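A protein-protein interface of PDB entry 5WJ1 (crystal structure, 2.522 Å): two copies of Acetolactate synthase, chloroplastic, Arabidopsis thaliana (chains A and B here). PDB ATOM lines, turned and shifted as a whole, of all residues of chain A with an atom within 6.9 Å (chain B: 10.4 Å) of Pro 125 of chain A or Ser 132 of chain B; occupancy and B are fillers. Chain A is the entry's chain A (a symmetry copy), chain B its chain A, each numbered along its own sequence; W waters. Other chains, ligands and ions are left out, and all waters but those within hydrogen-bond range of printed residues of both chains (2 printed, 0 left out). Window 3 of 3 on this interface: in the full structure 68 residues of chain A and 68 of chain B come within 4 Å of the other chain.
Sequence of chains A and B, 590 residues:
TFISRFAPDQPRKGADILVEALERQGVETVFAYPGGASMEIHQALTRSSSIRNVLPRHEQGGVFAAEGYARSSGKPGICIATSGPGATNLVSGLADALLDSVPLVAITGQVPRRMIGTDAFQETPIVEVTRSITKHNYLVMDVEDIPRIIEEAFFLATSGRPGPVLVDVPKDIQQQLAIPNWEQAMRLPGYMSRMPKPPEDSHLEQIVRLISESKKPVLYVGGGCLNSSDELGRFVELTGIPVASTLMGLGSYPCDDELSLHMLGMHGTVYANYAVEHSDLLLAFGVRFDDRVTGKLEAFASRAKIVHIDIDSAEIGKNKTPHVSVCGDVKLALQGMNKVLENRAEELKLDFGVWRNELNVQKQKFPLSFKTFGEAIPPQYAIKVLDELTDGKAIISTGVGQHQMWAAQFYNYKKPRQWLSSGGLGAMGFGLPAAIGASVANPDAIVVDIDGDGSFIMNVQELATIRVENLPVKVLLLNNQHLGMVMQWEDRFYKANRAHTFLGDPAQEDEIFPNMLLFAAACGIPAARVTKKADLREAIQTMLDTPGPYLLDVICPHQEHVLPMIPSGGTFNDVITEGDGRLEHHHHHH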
ATOM      1  N   GLN A 110      -3.346   1.153  -5.581  1.00  0.00           N
ATOM      2  CA  GLN A 110      -4.566   0.387  -5.362  1.00  0.00           C
ATOM      3  C   GLN A 110      -5.770   1.293  -5.582  1.00  0.00           C
ATOM      4  O   GLN A 110      -5.653   2.515  -5.485  1.00  0.00           O
ATOM      5  CB  GLN A 110      -4.571  -0.221  -3.952  1.00  0.00           C
ATOM      6  CG  GLN A 110      -5.803  -1.051  -3.578  1.00  0.00           C
ATOM      7  CD  GLN A 110      -6.075  -2.189  -4.548  1.00  0.00           C
ATOM      8  OE1 GLN A 110      -6.688  -1.994  -5.598  1.00  0.00           O
ATOM      9  NE2 GLN A 110      -5.621  -3.386  -4.197  1.00  0.00           N
ATOM     10  N   ILE A 116     -12.506  -1.246  -2.499  1.00  0.00           N
ATOM     11  CA  ILE A 116     -11.786  -2.503  -2.345  1.00  0.00           C
ATOM     12  C   ILE A 116     -12.759  -3.650  -2.098  1.00  0.00           C
ATOM     13  O   ILE A 116     -13.580  -3.594  -1.182  1.00  0.00           O
ATOM     14  CB  ILE A 116     -10.758  -2.424  -1.199  1.00  0.00           C
ATOM     15  CG1 ILE A 116      -9.684  -1.385  -1.532  1.00  0.00           C
ATOM     16  CG2 ILE A 116     -10.127  -3.789  -0.938  1.00  0.00           C
ATOM     17  CD1 ILE A 116      -8.620  -1.238  -0.473  1.00  0.00           C
ATOM     18  N   ASP A 119     -14.802  -5.634  -7.182  1.00  0.00           N
ATOM     19  CA  ASP A 119     -14.434  -5.901  -8.572  1.00  0.00           C
ATOM     20  C   ASP A 119     -14.331  -4.597  -9.360  1.00  0.00           C
ATOM     21  O   ASP A 119     -14.816  -4.498 -10.489  1.00  0.00           O
ATOM     22  CB  ASP A 119     -15.444  -6.841  -9.241  1.00  0.00           C
ATOM     23  CG  ASP A 119     -15.439  -8.231  -8.635  1.00  0.00           C
ATOM     24  OD1 ASP A 119     -14.451  -8.587  -7.958  1.00  0.00           O
ATOM     25  OD2 ASP A 119     -16.427  -8.968  -8.839  1.00  0.00           O
ATOM     26  N   GLU A 123      -8.819  -3.576 -10.345  1.00  0.00           N
ATOM     27  CA  GLU A 123      -8.633  -3.991  -8.963  1.00  0.00           C
ATOM     28  C   GLU A 123      -8.153  -5.430  -8.868  1.00  0.00           C
ATOM     29  O   GLU A 123      -8.717  -6.331  -9.487  1.00  0.00           O
ATOM     30  CB  GLU A 123      -9.922  -3.833  -8.152  1.00  0.00           C
ATOM     31  CG  GLU A 123      -9.733  -4.189  -6.679  1.00  0.00           C
ATOM     32  CD  GLU A 123     -11.039  -4.412  -5.935  1.00  0.00           C
ATOM     33  OE1 GLU A 123     -10.983  -4.858  -4.769  1.00  0.00           O
ATOM     34  OE2 GLU A 123     -12.115  -4.139  -6.507  1.00  0.00           O
ATOM     35  N   THR A 124      -7.105  -5.631  -8.083  1.00  0.00           N
ATOM     36  CA  THR A 124      -6.626  -6.964  -7.759  1.00  0.00           C
ATOM     37  C   THR A 124      -6.371  -7.027  -6.264  1.00  0.00           C
ATOM     38  O   THR A 124      -5.726  -6.138  -5.712  1.00  0.00           O
ATOM     39  CB  THR A 124      -5.333  -7.319  -8.532  1.00  0.00           C
ATOM     40  OG1 THR A 124      -5.607  -7.356  -9.937  1.00  0.00           O
ATOM     41  CG2 THR A 124      -4.805  -8.671  -8.101  1.00  0.00           C
ATOM     42  N   PRO A 125      -6.890  -8.068  -5.596  1.00  0.00           N
ATOM     43  CA  PRO A 125      -6.589  -8.260  -4.174  1.00  0.00           C
ATOM     44  C   PRO A 125      -5.139  -8.708  -3.984  1.00  0.00           C
ATOM     45  O   PRO A 125      -4.884  -9.856  -3.616  1.00  0.00           O
ATOM     46  CB  PRO A 125      -7.582  -9.349  -3.752  1.00  0.00           C
ATOM     47  CG  PRO A 125      -7.847 -10.117  -5.002  1.00  0.00           C
ATOM     48  CD  PRO A 125      -7.775  -9.119  -6.129  1.00  0.00           C
ATOM     49  N   ILE A 126      -4.204  -7.794  -4.234  1.00  0.00           N
ATOM     50  CA  ILE A 126      -2.794  -8.142  -4.372  1.00  0.00           C
ATOM     51  C   ILE A 126      -2.176  -8.594  -3.045  1.00  0.00           C
ATOM     52  O   ILE A 126      -1.240  -9.396  -3.036  1.00  0.00           O
ATOM     53  CB  ILE A 126      -1.979  -6.955  -4.963  1.00  0.00           C
ATOM     54  CG1 ILE A 126      -0.617  -7.430  -5.476  1.00  0.00           C
ATOM     55  CG2 ILE A 126      -1.826  -5.824  -3.960  1.00  0.00           C
ATOM     56  CD1 ILE A 126      -0.708  -8.468  -6.575  1.00  0.00           C
ATOM     57  N   VAL A 127      -2.709  -8.099  -1.931  1.00  0.00           N
ATOM     58  CA  VAL A 127      -2.240  -8.520  -0.614  1.00  0.00           C
ATOM     59  C   VAL A 127      -2.596  -9.989  -0.371  1.00  0.00           C
ATOM     60  O   VAL A 127      -1.788 -10.755   0.154  1.00  0.00           O
ATOM     61  CB  VAL A 127      -2.823  -7.627   0.505  1.00  0.00           C
ATOM     62  CG1 VAL A 127      -2.684  -8.291   1.862  1.00  0.00           C
ATOM     63  CG2 VAL A 127      -2.131  -6.272   0.508  1.00  0.00           C
ATOM     64  N   GLU A 128      -3.802 -10.377  -0.775  1.00  0.00           N
ATOM     65  CA  GLU A 128      -4.237 -11.772  -0.718  1.00  0.00           C
ATOM     66  C   GLU A 128      -3.389 -12.662  -1.624  1.00  0.00           C
ATOM     67  O   GLU A 128      -2.901 -13.715  -1.211  1.00  0.00           O
ATOM     68  CB  GLU A 128      -5.711 -11.885  -1.117  1.00  0.00           C
ATOM     69  CG  GLU A 128      -6.665 -12.110   0.038  1.00  0.00           C
ATOM     70  CD  GLU A 128      -6.607 -13.529   0.562  1.00  0.00           C
ATOM     71  OE1 GLU A 128      -6.777 -14.467  -0.246  1.00  0.00           O
ATOM     72  OE2 GLU A 128      -6.389 -13.706   1.780  1.00  0.00           O
ATOM     73  N   VAL A 129      -3.224 -12.222  -2.866  1.00  0.00           N
ATOM     74  CA  VAL A 129      -2.490 -12.971  -3.878  1.00  0.00           C
ATOM     75  C   VAL A 129      -1.034 -13.227  -3.480  1.00  0.00           C
ATOM     76  O   VAL A 129      -0.515 -14.330  -3.669  1.00  0.00           O
ATOM     77  CB  VAL A 129      -2.524 -12.224  -5.236  1.00  0.00           C
ATOM     78  CG1 VAL A 129      -1.561 -12.847  -6.232  1.00  0.00           C
ATOM     79  CG2 VAL A 129      -3.942 -12.201  -5.791  1.00  0.00           C
ATOM     80  N   THR A 130      -0.385 -12.218  -2.908  1.00  0.00           N
ATOM     81  CA  THR A 130       1.051 -12.286  -2.666  1.00  0.00           C
ATOM     82  C   THR A 130       1.440 -12.626  -1.230  1.00  0.00           C
ATOM     83  O   THR A 130       2.616 -12.567  -0.878  1.00  0.00           O
ATOM     84  CB  THR A 130       1.735 -10.954  -3.034  1.00  0.00           C
ATOM     85  OG1 THR A 130       1.271  -9.916  -2.163  1.00  0.00           O
ATOM     86  CG2 THR A 130       1.434 -10.580  -4.474  1.00  0.00           C
ATOM     87  N   ASP A 168       0.777  -2.029  -0.399  1.00  0.00           N
ATOM     88  CA  ASP A 168      -0.344  -1.664  -1.264  1.00  0.00           C
ATOM     89  C   ASP A 168      -0.965  -0.336  -0.823  1.00  0.00           C
ATOM     90  O   ASP A 168      -1.417  -0.206   0.316  1.00  0.00           O
ATOM     91  CB  ASP A 168      -1.399  -2.777  -1.258  1.00  0.00           C
ATOM     92  CG  ASP A 168      -2.306  -2.739  -2.475  1.00  0.00           C
ATOM     93  OD1 ASP A 168      -1.842  -2.320  -3.556  1.00  0.00           O
ATOM     94  OD2 ASP A 168      -3.482  -3.143  -2.354  1.00  0.00           O
ATOM     95  N   VAL B  91      -0.608 -15.458 -13.969  1.00  0.00           N
ATOM     96  CA  VAL B  91      -1.445 -14.747 -12.998  1.00  0.00           C
ATOM     97  C   VAL B  91      -2.259 -13.576 -13.575  1.00  0.00           C
ATOM     98  O   VAL B  91      -3.460 -13.476 -13.319  1.00  0.00           O
ATOM     99  CB  VAL B  91      -0.581 -14.243 -11.817  1.00  0.00           C
ATOM    100  CG1 VAL B  91      -1.317 -13.195 -11.004  1.00  0.00           C
ATOM    101  CG2 VAL B  91      -0.180 -15.414 -10.934  1.00  0.00           C
ATOM    102  N   LEU B  94      -5.188 -14.928 -15.579  1.00  0.00           N
ATOM    103  CA  LEU B  94      -6.233 -15.497 -14.736  1.00  0.00           C
ATOM    104  C   LEU B  94      -7.130 -14.399 -14.175  1.00  0.00           C
ATOM    105  O   LEU B  94      -8.357 -14.488 -14.245  1.00  0.00           O
ATOM    106  CB  LEU B  94      -5.620 -16.318 -13.598  1.00  0.00           C
ATOM    107  CG  LEU B  94      -4.746 -17.498 -14.024  1.00  0.00           C
ATOM    108  CD1 LEU B  94      -4.149 -18.196 -12.812  1.00  0.00           C
ATOM    109  CD2 LEU B  94      -5.560 -18.471 -14.854  1.00  0.00           C
ATOM    110  N   ALA B  95      -6.508 -13.360 -13.624  1.00  0.00           N
ATOM    111  CA  ALA B  95      -7.247 -12.231 -13.073  1.00  0.00           C
ATOM    112  C   ALA B  95      -8.059 -11.530 -14.159  1.00  0.00           C
ATOM    113  O   ALA B  95      -9.187 -11.098 -13.921  1.00  0.00           O
ATOM    114  CB  ALA B  95      -6.297 -11.250 -12.403  1.00  0.00           C
ATOM    115  N   ASP B  96      -7.477 -11.432 -15.349  1.00  0.00           N
ATOM    116  CA  ASP B  96      -8.131 -10.794 -16.486  1.00  0.00           C
ATOM    117  C   ASP B  96      -9.393 -11.552 -16.891  1.00  0.00           C
ATOM    118  O   ASP B  96     -10.443 -10.951 -17.115  1.00  0.00           O
ATOM    119  CB  ASP B  96      -7.162 -10.697 -17.668  1.00  0.00           C
ATOM    120  CG  ASP B  96      -7.669  -9.787 -18.769  1.00  0.00           C
ATOM    121  OD1 ASP B  96      -8.244  -8.724 -18.452  1.00  0.00           O
ATOM    122  OD2 ASP B  96      -7.484 -10.130 -19.954  1.00  0.00           O
ATOM    123  N   ALA B  97      -9.286 -12.875 -16.967  1.00  0.00           N
ATOM    124  CA  ALA B  97     -10.416 -13.716 -17.352  1.00  0.00           C
ATOM    125  C   ALA B  97     -11.526 -13.710 -16.299  1.00  0.00           C
ATOM    126  O   ALA B  97     -12.702 -13.842 -16.635  1.00  0.00           O
ATOM    127  CB  ALA B  97      -9.950 -15.140 -17.615  1.00  0.00           C
ATOM    128  N   LEU B  98     -11.157 -13.560 -15.031  1.00  0.00           N
ATOM    129  CA  LEU B  98     -12.153 -13.517 -13.964  1.00  0.00           C
ATOM    130  C   LEU B  98     -12.956 -12.222 -14.019  1.00  0.00           C
ATOM    131  O   LEU B  98     -14.185 -12.243 -13.945  1.00  0.00           O
ATOM    132  CB  LEU B  98     -11.495 -13.668 -12.588  1.00  0.00           C
ATOM    133  CG  LEU B  98     -12.460 -13.562 -11.398  1.00  0.00           C
ATOM    134  CD1 LEU B  98     -13.519 -14.660 -11.446  1.00  0.00           C
ATOM    135  CD2 LEU B  98     -11.719 -13.594 -10.068  1.00  0.00           C
ATOM    136  N   LEU B  99     -12.260 -11.100 -14.156  1.00  0.00           N
ATOM    137  CA  LEU B  99     -12.919  -9.802 -14.178  1.00  0.00           C
ATOM    138  C   LEU B  99     -13.808  -9.627 -15.412  1.00  0.00           C
ATOM    139  O   LEU B  99     -14.834  -8.955 -15.344  1.00  0.00           O
ATOM    140  CB  LEU B  99     -11.882  -8.680 -14.105  1.00  0.00           C
ATOM    141  CG  LEU B  99     -11.391  -8.354 -12.693  1.00  0.00           C
ATOM    142  CD1 LEU B  99     -10.340  -7.262 -12.716  1.00  0.00           C
ATOM    143  CD2 LEU B  99     -12.559  -7.938 -11.821  1.00  0.00           C
ATOM    144  N   PRO B 125       3.126 -21.969  -4.279  1.00  0.00           N
ATOM    145  CA  PRO B 125       1.792 -22.341  -3.799  1.00  0.00           C
ATOM    146  C   PRO B 125       0.708 -21.692  -4.662  1.00  0.00           C
ATOM    147  O   PRO B 125       0.004 -20.789  -4.206  1.00  0.00           O
ATOM    148  CB  PRO B 125       1.774 -21.804  -2.364  1.00  0.00           C
ATOM    149  CG  PRO B 125       2.729 -20.658  -2.383  1.00  0.00           C
ATOM    150  CD  PRO B 125       3.806 -21.029  -3.369  1.00  0.00           C
ATOM    151  N   ILE B 126       0.582 -22.165  -5.901  1.00  0.00           N
ATOM    152  CA  ILE B 126      -0.198 -21.473  -6.921  1.00  0.00           C
ATOM    153  C   ILE B 126      -1.701 -21.504  -6.622  1.00  0.00           C
ATOM    154  O   ILE B 126      -2.431 -20.589  -7.009  1.00  0.00           O
ATOM    155  CB  ILE B 126       0.076 -22.064  -8.334  1.00  0.00           C
ATOM    156  CG1 ILE B 126      -0.412 -21.111  -9.428  1.00  0.00           C
ATOM    157  CG2 ILE B 126      -0.536 -23.446  -8.492  1.00  0.00           C
ATOM    158  CD1 ILE B 126       0.261 -19.756  -9.400  1.00  0.00           C
ATOM    159  N   VAL B 127      -2.156 -22.539  -5.919  1.00  0.00           N
ATOM    160  CA  VAL B 127      -3.558 -22.627  -5.521  1.00  0.00           C
ATOM    161  C   VAL B 127      -3.887 -21.533  -4.501  1.00  0.00           C
ATOM    162  O   VAL B 127      -4.941 -20.901  -4.574  1.00  0.00           O
ATOM    163  CB  VAL B 127      -3.894 -24.023  -4.947  1.00  0.00           C
ATOM    164  CG1 VAL B 127      -5.196 -23.993  -4.167  1.00  0.00           C
ATOM    165  CG2 VAL B 127      -3.977 -25.045  -6.071  1.00  0.00           C
ATOM    166  N   GLU B 128      -2.969 -21.302  -3.568  1.00  0.00           N
ATOM    167  CA  GLU B 128      -3.091 -20.211  -2.601  1.00  0.00           C
ATOM    168  C   GLU B 128      -3.072 -18.847  -3.289  1.00  0.00           C
ATOM    169  O   GLU B 128      -3.922 -17.992  -3.037  1.00  0.00           O
ATOM    170  CB  GLU B 128      -1.960 -20.286  -1.573  1.00  0.00           C
ATOM    171  CG  GLU B 128      -2.373 -20.808  -0.212  1.00  0.00           C
ATOM    172  CD  GLU B 128      -3.149 -19.780   0.585  1.00  0.00           C
ATOM    173  OE1 GLU B 128      -2.636 -18.655   0.761  1.00  0.00           O
ATOM    174  OE2 GLU B 128      -4.273 -20.098   1.031  1.00  0.00           O
ATOM    175  N   VAL B 129      -2.088 -18.659  -4.160  1.00  0.00           N
ATOM    176  CA  VAL B 129      -1.888 -17.400  -4.867  1.00  0.00           C
ATOM    177  C   VAL B 129      -3.095 -17.008  -5.723  1.00  0.00           C
ATOM    178  O   VAL B 129      -3.501 -15.844  -5.742  1.00  0.00           O
ATOM    179  CB  VAL B 129      -0.627 -17.478  -5.765  1.00  0.00           C
ATOM    180  CG1 VAL B 129      -0.542 -16.281  -6.697  1.00  0.00           C
ATOM    181  CG2 VAL B 129       0.627 -17.590  -4.909  1.00  0.00           C
ATOM    182  N   THR B 130      -3.680 -17.983  -6.412  1.00  0.00           N
ATOM    183  CA  THR B 130      -4.708 -17.692  -7.404  1.00  0.00           C
ATOM    184  C   THR B 130      -6.139 -17.920  -6.923  1.00  0.00           C
ATOM    185  O   THR B 130      -7.075 -17.848  -7.717  1.00  0.00           O
ATOM    186  CB  THR B 130      -4.501 -18.537  -8.677  1.00  0.00           C
ATOM    187  OG1 THR B 130      -4.677 -19.924  -8.369  1.00  0.00           O
ATOM    188  CG2 THR B 130      -3.109 -18.315  -9.242  1.00  0.00           C
ATOM    189  N   ARG B 131      -6.314 -18.190  -5.633  1.00  0.00           N
ATOM    190  CA  ARG B 131      -7.643 -18.476  -5.102  1.00  0.00           C
ATOM    191  C   ARG B 131      -8.599 -17.292  -5.258  1.00  0.00           C
ATOM    192  O   ARG B 131      -9.771 -17.470  -5.585  1.00  0.00           O
ATOM    193  CB  ARG B 131      -7.566 -18.880  -3.627  1.00  0.00           C
ATOM    194  CG  ARG B 131      -8.908 -19.337  -3.066  1.00  0.00           C
ATOM    195  CD  ARG B 131      -8.807 -19.812  -1.623  1.00  0.00           C
ATOM    196  NE  ARG B 131      -8.058 -21.060  -1.504  1.00  0.00           N
ATOM    197  CZ  ARG B 131      -6.882 -21.173  -0.892  1.00  0.00           C
ATOM    198  NH1 ARG B 131      -6.272 -22.349  -0.835  1.00  0.00           N
ATOM    199  NH2 ARG B 131      -6.317 -20.110  -0.331  1.00  0.00           N
ATOM    200  N   SER B 132      -8.093 -16.085  -5.034  1.00  0.00           N
ATOM    201  CA  SER B 132      -8.931 -14.895  -5.094  1.00  0.00           C
ATOM    202  C   SER B 132      -9.042 -14.310  -6.503  1.00  0.00           C
ATOM    203  O   SER B 132      -9.757 -13.329  -6.712  1.00  0.00           O
ATOM    204  CB  SER B 132      -8.401 -13.828  -4.133  1.00  0.00           C
ATOM    205  OG  SER B 132      -7.164 -13.303  -4.583  1.00  0.00           O
ATOM    206  N   ILE B 133      -8.340 -14.908  -7.463  1.00  0.00           N
ATOM    207  CA  ILE B 133      -8.386 -14.428  -8.843  1.00  0.00           C
ATOM    208  C   ILE B 133      -8.750 -15.526  -9.842  1.00  0.00           C
ATOM    209  O   ILE B 133      -8.430 -15.430 -11.025  1.00  0.00           O
ATOM    210  CB  ILE B 133      -7.046 -13.795  -9.270  1.00  0.00           C
ATOM    211  CG1 ILE B 133      -5.882 -14.726  -8.939  1.00  0.00           C
ATOM    212  CG2 ILE B 133      -6.859 -12.447  -8.595  1.00  0.00           C
ATOM    213  CD1 ILE B 133      -4.569 -14.304  -9.560  1.00  0.00           C
ATOM    214  N   THR B 134      -9.416 -16.568  -9.357  1.00  0.00           N
ATOM    215  CA  THR B 134     -10.020 -17.571 -10.231  1.00  0.00           C
ATOM    216  C   THR B 134     -11.452 -17.836  -9.777  1.00  0.00           C
ATOM    217  O   THR B 134     -11.819 -17.522  -8.645  1.00  0.00           O
ATOM    218  CB  THR B 134      -9.225 -18.896 -10.244  1.00  0.00           C
ATOM    219  OG1 THR B 134      -9.064 -19.378  -8.905  1.00  0.00           O
ATOM    220  CG2 THR B 134      -7.855 -18.700 -10.882  1.00  0.00           C
ATOM    221  N   LYS B 135     -12.264 -18.399 -10.664  1.00  0.00           N
ATOM    222  CA  LYS B 135     -13.626 -18.764 -10.298  1.00  0.00           C
ATOM    223  C   LYS B 135     -13.560 -19.927  -9.322  1.00  0.00           C
ATOM    224  O   LYS B 135     -14.348 -20.018  -8.378  1.00  0.00           O
ATOM    225  CB  LYS B 135     -14.453 -19.132 -11.531  1.00  0.00           C
ATOM    226  CG  LYS B 135     -15.871 -19.578 -11.214  1.00  0.00           C
ATOM    227  CD  LYS B 135     -16.684 -19.814 -12.475  1.00  0.00           C
ATOM    228  CE  LYS B 135     -18.105 -20.238 -12.134  1.00  0.00           C
ATOM    229  NZ  LYS B 135     -18.952 -20.413 -13.350  1.00  0.00           N
ATOM    230  N   HIS B 136     -12.595 -20.806  -9.568  1.00  0.00           N
ATOM    231  CA  HIS B 136     -12.321 -21.949  -8.712  1.00  0.00           C
ATOM    232  C   HIS B 136     -10.964 -22.530  -9.099  1.00  0.00           C
ATOM    233  O   HIS B 136     -10.468 -22.266 -10.193  1.00  0.00           O
ATOM    234  CB  HIS B 136     -13.423 -23.004  -8.843  1.00  0.00           C
ATOM    235  CG  HIS B 136     -13.457 -23.986  -7.713  1.00  0.00           C
ATOM    236  ND1 HIS B 136     -13.387 -25.348  -7.909  1.00  0.00           N
ATOM    237  CD2 HIS B 136     -13.554 -23.801  -6.376  1.00  0.00           C
ATOM    238  CE1 HIS B 136     -13.441 -25.962  -6.740  1.00  0.00           C
ATOM    239  NE2 HIS B 136     -13.540 -25.046  -5.794  1.00  0.00           N
ATOM    240  N   ASN B 137     -10.354 -23.301  -8.203  1.00  0.00           N
ATOM    241  CA  ASN B 137      -9.133 -24.020  -8.554  1.00  0.00           C
ATOM    242  C   ASN B 137      -8.981 -25.324  -7.781  1.00  0.00           C
ATOM    243  O   ASN B 137      -9.702 -25.572  -6.814  1.00  0.00           O
ATOM    244  CB  ASN B 137      -7.890 -23.133  -8.358  1.00  0.00           C
ATOM    245  CG  ASN B 137      -7.728 -22.625  -6.932  1.00  0.00           C
ATOM    246  OD1 ASN B 137      -8.303 -23.162  -5.986  1.00  0.00           O
ATOM    247  ND2 ASN B 137      -6.919 -21.583  -6.776  1.00  0.00           N
ATOM    248  N   PRO B 164     -12.222 -18.339 -15.197  1.00  0.00           N
ATOM    249  CA  PRO B 164     -11.041 -19.203 -15.214  1.00  0.00           C
ATOM    250  C   PRO B 164     -11.031 -20.218 -14.074  1.00  0.00           C
ATOM    251  O   PRO B 164     -11.358 -19.881 -12.936  1.00  0.00           O
ATOM    252  CB  PRO B 164      -9.887 -18.211 -15.068  1.00  0.00           C
ATOM    253  CG  PRO B 164     -10.467 -17.099 -14.274  1.00  0.00           C
ATOM    254  CD  PRO B 164     -11.911 -16.990 -14.693  1.00  0.00           C
ATOM    255  N   LEU B 166      -8.257 -23.068 -12.451  1.00  0.00           N
ATOM    256  CA  LEU B 166      -6.889 -23.580 -12.492  1.00  0.00           C
ATOM    257  C   LEU B 166      -6.789 -24.965 -11.865  1.00  0.00           C
ATOM    258  O   LEU B 166      -7.350 -25.220 -10.803  1.00  0.00           O
ATOM    259  CB  LEU B 166      -5.928 -22.618 -11.789  1.00  0.00           C
ATOM    260  CG  LEU B 166      -4.447 -23.011 -11.776  1.00  0.00           C
ATOM    261  CD1 LEU B 166      -3.577 -21.785 -11.977  1.00  0.00           C
ATOM    262  CD2 LEU B 166      -4.064 -23.717 -10.477  1.00  0.00           C
ATOM    263  N   LEU B 425      -9.888  -5.680 -15.916  1.00  0.00           N
ATOM    264  CA  LEU B 425      -8.530  -5.541 -15.413  1.00  0.00           C
ATOM    265  C   LEU B 425      -7.768  -4.508 -16.236  1.00  0.00           C
ATOM    266  O   LEU B 425      -6.943  -3.764 -15.703  1.00  0.00           O
ATOM    267  CB  LEU B 425      -7.806  -6.889 -15.437  1.00  0.00           C
ATOM    268  CG  LEU B 425      -6.425  -6.954 -14.786  1.00  0.00           C
ATOM    269  CD1 LEU B 425      -6.535  -6.780 -13.276  1.00  0.00           C
ATOM    270  CD2 LEU B 425      -5.730  -8.261 -15.134  1.00  0.00           C
HETATM  271  O   HOH W   1      -3.032 -16.074   0.543  1.00  0.00           O
HETATM  272  O   HOH W   2      -5.777 -16.718  -1.141  1.00  0.00           O
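The backbone carbonyl oxygen (O) of Thr 124 of chain A sits at hydrogen-bond distance from the side-chain amide nitrogen (NE2) of Gln 110 of chain A (3.1 Å). The backbone NH (N) of Asp 119 of chain A lies within hydrogen-bond range of the side-chain carboxylate (OE2) of Glu 123 of chain A, at 3.1 Å.
Among the printed residues, pairs that only touch across the chains: Glu 123 of chain A with Leu 99 of chain B (3.7 Å), Thr 124 of chain A with Leu 425 of chain B (3.5 Å), Pro 125 of chain A with Ser 132 of chain B (3.3 Å), Val 129 of chain A with Val 129 of chain B (3.6 Å) and Val 129 of chain A with Ser 132 of chain B (3.6 Å).
Printed residues of chain B within 4 Å of Pro 125 of chain A: Ser 132 (3.3 Å). Of chain B, only Leu 425 comes within 4 Å of Thr 124 of chain A. No residue of chain B comes within 4 Å of Ile 126 of chain A. Of chain B, only Val 129 (3.6 Å) and Ser 132 (3.6 Å) come within 4 Å of Val 129 of chain A. Printed residues of chain A within 4 Å of Val 129 of chain B: Val 129 (3.6 Å). Of the printed residues of chain B, Glu 123 of chain A touches Leu 99 (3.7 Å). Ile 126 of chain B touches none of the printed residues of chain A. Thr 130 of chain B touches none of the printed residues of chain A. The nearest printed residue of chain A that does not touch Ser 132 of chain B is Glu 128 of chain A (4.02 Å).
Hydrophobic or aromatic side chains of chain A that line the printed part of chain B: Pro 125 and Val 129. Among the printed residues, 5 pairs touch across the chains. Among the printed residues, no Asp or Glu carboxylate lies within 4 Å of a Lys or Arg side-chain nitrogen of the other chain.
Val 129 of chain B touches its own counterpart, Val 129 of chain A.
Water W1 lies within hydrogen-bond range of OE1 of Glu 128 of chain B and O of Glu 128 of chain A. Water W2 bridges OE1 of Glu 128 of chain A (2.6 Å) and O of Glu 128 of chain B (2.9 Å).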
